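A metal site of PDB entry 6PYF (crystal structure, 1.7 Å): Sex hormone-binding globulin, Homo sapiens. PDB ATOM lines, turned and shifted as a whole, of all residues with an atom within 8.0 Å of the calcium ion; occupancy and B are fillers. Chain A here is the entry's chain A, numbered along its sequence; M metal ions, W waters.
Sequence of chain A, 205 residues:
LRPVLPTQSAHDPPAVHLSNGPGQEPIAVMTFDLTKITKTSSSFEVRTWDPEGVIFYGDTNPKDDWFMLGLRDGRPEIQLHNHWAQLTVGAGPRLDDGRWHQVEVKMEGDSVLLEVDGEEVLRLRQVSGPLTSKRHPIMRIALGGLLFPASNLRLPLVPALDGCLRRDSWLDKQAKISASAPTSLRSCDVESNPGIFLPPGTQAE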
ATOM      1  N   SER A  19     -10.067   8.824 -27.261  1.00  0.00           N
ATOM      2  CA  SER A  19      -9.956   7.422 -26.905  1.00  0.00           C
ATOM      3  C   SER A  19     -10.192   6.602 -28.163  1.00  0.00           C
ATOM      4  O   SER A  19     -10.951   6.997 -29.052  1.00  0.00           O
ATOM      5  CB  SER A  19     -10.951   7.021 -25.810  1.00  0.00           C
ATOM      6  OG  SER A  19     -10.736   7.838 -24.659  1.00  0.00           O
ATOM      7  N   THR A  48     -16.860  17.116 -25.625  1.00  0.00           N
ATOM      8  CA  THR A  48     -17.223  15.817 -25.083  1.00  0.00           C
ATOM      9  C   THR A  48     -18.592  15.894 -24.415  1.00  0.00           C
ATOM     10  O   THR A  48     -19.000  16.945 -23.929  1.00  0.00           O
ATOM     11  CB  THR A  48     -16.182  15.330 -24.078  1.00  0.00           C
ATOM     12  OG1 THR A  48     -16.476  14.007 -23.648  1.00  0.00           O
ATOM     13  CG2 THR A  48     -16.143  16.237 -22.828  1.00  0.00           C
ATOM     14  N   TRP A  49     -19.263  14.752 -24.388  1.00  0.00           N
ATOM     15  CA  TRP A  49     -20.416  14.514 -23.524  1.00  0.00           C
ATOM     16  C   TRP A  49     -20.068  13.621 -22.326  1.00  0.00           C
ATOM     17  O   TRP A  49     -20.975  13.244 -21.577  1.00  0.00           O
ATOM     18  CB  TRP A  49     -21.552  13.867 -24.330  1.00  0.00           C
ATOM     19  CG  TRP A  49     -22.111  14.742 -25.411  1.00  0.00           C
ATOM     20  CD1 TRP A  49     -21.748  14.748 -26.729  1.00  0.00           C
ATOM     21  CD2 TRP A  49     -23.117  15.735 -25.258  1.00  0.00           C
ATOM     22  NE1 TRP A  49     -22.491  15.694 -27.412  1.00  0.00           N
ATOM     23  CE2 TRP A  49     -23.339  16.306 -26.529  1.00  0.00           C
ATOM     24  CE3 TRP A  49     -23.867  16.202 -24.182  1.00  0.00           C
ATOM     25  CZ2 TRP A  49     -24.264  17.319 -26.744  1.00  0.00           C
ATOM     26  CZ3 TRP A  49     -24.785  17.218 -24.390  1.00  0.00           C
ATOM     27  CH2 TRP A  49     -24.987  17.754 -25.666  1.00  0.00           C
ATOM     28  N   ASP A  50     -18.779  13.295 -22.168  1.00  0.00           N
ATOM     29  CA  ASP A  50     -18.304  12.342 -21.163  1.00  0.00           C
ATOM     30  C   ASP A  50     -17.941  13.082 -19.892  1.00  0.00           C
ATOM     31  O   ASP A  50     -17.163  14.038 -19.957  1.00  0.00           O
ATOM     32  CB  ASP A  50     -17.079  11.610 -21.723  1.00  0.00           C
ATOM     33  CG  ASP A  50     -16.615  10.441 -20.877  1.00  0.00           C
ATOM     34  OD1 ASP A  50     -16.972  10.334 -19.694  1.00  0.00           O
ATOM     35  OD2 ASP A  50     -15.835   9.609 -21.424  1.00  0.00           O
ATOM     36  N   PRO A  51     -18.497  12.718 -18.735  1.00  0.00           N
ATOM     37  CA  PRO A  51     -18.193  13.456 -17.494  1.00  0.00           C
ATOM     38  C   PRO A  51     -16.860  13.098 -16.852  1.00  0.00           C
ATOM     39  O   PRO A  51     -16.438  13.798 -15.918  1.00  0.00           O
ATOM     40  CB  PRO A  51     -19.355  13.080 -16.565  1.00  0.00           C
ATOM     41  CG  PRO A  51     -19.735  11.697 -17.025  1.00  0.00           C
ATOM     42  CD  PRO A  51     -19.485  11.641 -18.498  1.00  0.00           C
ATOM     43  N   GLU A  52     -16.158  12.070 -17.334  1.00  0.00           N
ATOM     44  CA  GLU A  52     -14.999  11.590 -16.597  1.00  0.00           C
ATOM     45  C   GLU A  52     -13.953  11.036 -17.558  1.00  0.00           C
ATOM     46  O   GLU A  52     -14.296  10.301 -18.496  1.00  0.00           O
ATOM     47  CB  GLU A  52     -15.390  10.510 -15.592  1.00  0.00           C
ATOM     48  CG  GLU A  52     -14.226  10.039 -14.721  1.00  0.00           C
ATOM     49  CD  GLU A  52     -14.657   9.154 -13.600  1.00  0.00           C
ATOM     50  OE1 GLU A  52     -15.656   9.496 -12.925  1.00  0.00           O
ATOM     51  OE2 GLU A  52     -13.996   8.120 -13.360  1.00  0.00           O
ATOM     52  N   GLY A  53     -12.712  11.389 -17.329  1.00  0.00           N
ATOM     53  CA  GLY A  53     -11.631  10.845 -18.141  1.00  0.00           C
ATOM     54  C   GLY A  53     -10.414  11.734 -18.117  1.00  0.00           C
ATOM     55  O   GLY A  53     -10.405  12.816 -17.535  1.00  0.00           O
ATOM     56  N   VAL A  54      -9.347  11.227 -18.747  1.00  0.00           N
ATOM     57  CA  VAL A  54      -8.089  11.963 -18.857  1.00  0.00           C
ATOM     58  C   VAL A  54      -8.067  12.752 -20.143  1.00  0.00           C
ATOM     59  O   VAL A  54      -8.350  12.223 -21.232  1.00  0.00           O
ATOM     60  CB  VAL A  54      -6.873  11.017 -18.796  1.00  0.00           C
ATOM     61  CG1 VAL A  54      -5.562  11.771 -19.104  1.00  0.00           C
ATOM     62  CG2 VAL A  54      -6.777  10.337 -17.479  1.00  0.00           C
ATOM     63  N   LEU A  71     -11.298  15.245 -16.526  1.00  0.00           N
ATOM     64  CA  LEU A  71     -12.623  15.635 -16.078  1.00  0.00           C
ATOM     65  C   LEU A  71     -13.129  14.664 -15.024  1.00  0.00           C
ATOM     66  O   LEU A  71     -12.865  13.456 -15.100  1.00  0.00           O
ATOM     67  CB  LEU A  71     -13.613  15.651 -17.256  1.00  0.00           C
ATOM     68  CG  LEU A  71     -13.319  16.623 -18.398  1.00  0.00           C
ATOM     69  CD1 LEU A  71     -14.428  16.497 -19.436  1.00  0.00           C
ATOM     70  CD2 LEU A  71     -13.223  18.024 -17.852  1.00  0.00           C
ATOM     71  N   LEU A 157      -9.638   7.742 -11.295  1.00  0.00           N
ATOM     72  CA  LEU A 157     -10.773   7.871 -12.184  1.00  0.00           C
ATOM     73  C   LEU A 157     -10.602   6.846 -13.297  1.00  0.00           C
ATOM     74  O   LEU A 157      -9.554   6.191 -13.410  1.00  0.00           O
ATOM     75  CB  LEU A 157     -10.922   9.290 -12.726  1.00  0.00           C
ATOM     76  CG  LEU A 157      -9.697  10.010 -13.281  1.00  0.00           C
ATOM     77  CD1 LEU A 157      -9.144   9.341 -14.548  1.00  0.00           C
ATOM     78  CD2 LEU A 157     -10.066  11.480 -13.567  1.00  0.00           C
ATOM     79  N   VAL A 158     -11.644   6.662 -14.091  1.00  0.00           N
ATOM     80  CA  VAL A 158     -11.588   5.805 -15.264  1.00  0.00           C
ATOM     81  C   VAL A 158     -11.082   6.652 -16.425  1.00  0.00           C
ATOM     82  O   VAL A 158     -11.763   7.617 -16.804  1.00  0.00           O
ATOM     83  CB  VAL A 158     -12.948   5.178 -15.587  1.00  0.00           C
ATOM     84  CG1 VAL A 158     -12.853   4.340 -16.860  1.00  0.00           C
ATOM     85  CG2 VAL A 158     -13.433   4.317 -14.425  1.00  0.00           C
ATOM     86  N   PRO A 159      -9.912   6.357 -17.007  1.00  0.00           N
ATOM     87  CA  PRO A 159      -9.256   7.351 -17.855  1.00  0.00           C
ATOM     88  C   PRO A 159      -9.920   7.607 -19.188  1.00  0.00           C
ATOM     89  O   PRO A 159      -9.706   8.678 -19.756  1.00  0.00           O
ATOM     90  CB  PRO A 159      -7.838   6.796 -18.052  1.00  0.00           C
ATOM     91  CG  PRO A 159      -7.682   5.725 -17.060  1.00  0.00           C
ATOM     92  CD  PRO A 159      -9.040   5.200 -16.715  1.00  0.00           C
ATOM     93  N   ALA A 160     -10.695   6.661 -19.712  1.00  0.00           N
ATOM     94  CA  ALA A 160     -11.237   6.812 -21.060  1.00  0.00           C
ATOM     95  C   ALA A 160     -12.126   8.036 -21.164  1.00  0.00           C
ATOM     96  O   ALA A 160     -13.136   8.163 -20.451  1.00  0.00           O
ATOM     97  CB  ALA A 160     -12.020   5.560 -21.469  1.00  0.00           C
ATOM     98  N   LEU A 161     -11.735   8.952 -22.047  1.00  0.00           N
ATOM     99  CA  LEU A 161     -12.502  10.170 -22.306  1.00  0.00           C
ATOM    100  C   LEU A 161     -13.026  10.088 -23.733  1.00  0.00           C
ATOM    101  O   LEU A 161     -12.246  10.194 -24.682  1.00  0.00           O
ATOM    102  CB  LEU A 161     -11.676  11.426 -22.109  1.00  0.00           C
ATOM    103  CG  LEU A 161     -12.520  12.693 -22.116  1.00  0.00           C
ATOM    104  CD1 LEU A 161     -13.518  12.710 -20.985  1.00  0.00           C
ATOM    105  CD2 LEU A 161     -11.622  13.916 -22.029  1.00  0.00           C
ATOM    106  N   ASP A 162     -14.328   9.920 -23.866  1.00  0.00           N
ATOM    107  CA  ASP A 162     -14.975   9.863 -25.176  1.00  0.00           C
ATOM    108  C   ASP A 162     -15.184  11.286 -25.648  1.00  0.00           C
ATOM    109  O   ASP A 162     -16.232  11.901 -25.477  1.00  0.00           O
ATOM    110  CB  ASP A 162     -16.292   9.105 -25.088  1.00  0.00           C
ATOM    111  CG  ASP A 162     -16.908   8.843 -26.444  1.00  0.00           C
ATOM    112  OD1 ASP A 162     -16.311   9.240 -27.467  1.00  0.00           O
ATOM    113  OD2 ASP A 162     -18.002   8.213 -26.486  1.00  0.00           O
ATOM    114  N   GLY A 163     -14.120  11.849 -26.219  1.00  0.00           N
ATOM    115  CA  GLY A 163     -14.156  13.230 -26.666  1.00  0.00           C
ATOM    116  C   GLY A 163     -13.244  13.446 -27.852  1.00  0.00           C
ATOM    117  O   GLY A 163     -12.597  12.526 -28.340  1.00  0.00           O
HETATM  118 CA    CA M   1     -15.265   8.488 -19.503  1.00  0.00          CA
HETATM  119  O   HOH W   1     -14.402   7.490 -17.689  1.00  0.00           O
HETATM  120  O   HOH W   2     -17.157   7.865 -18.170  1.00  0.00           O
HETATM  121  O   HOH W   3     -16.027   6.599 -20.941  1.00  0.00           O
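Three residues have an atom within 4 Å of the calcium ion: Asp 50, Glu 52 and Ala 160.
Along chain A the residues within 4 Å of the calcium ion span positions 50 to 160.
The nearest printed residue that does not touch the calcium ion is Leu 161 (4.3 Å).
The backbone NH (N) of Val 158 is in hydrogen-bond range of the side-chain carboxylate (OE2) of Glu 52 (2.9 Å).
The backbone NH (N) of Asp 162 sits close to the side-chain carboxylate (OD2) of Asp 50 (2.9 Å).
The backbone NH of Asp 50 sits at hydrogen-bond distance from the side-chain hydroxyl of Thr 48.
The calcium ion is bound by water W1 (2.2 Å), O of Glu 52 (2.3 Å), OD2 of Asp 50 (2.3 Å), O of Ala 160 (2.4 Å), water W2 (2.4 Å), water W3 (2.5 Å) and OD1 of Asp 50 (2.5 Å).
The calcium ion has seven donor atoms within binding distance.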
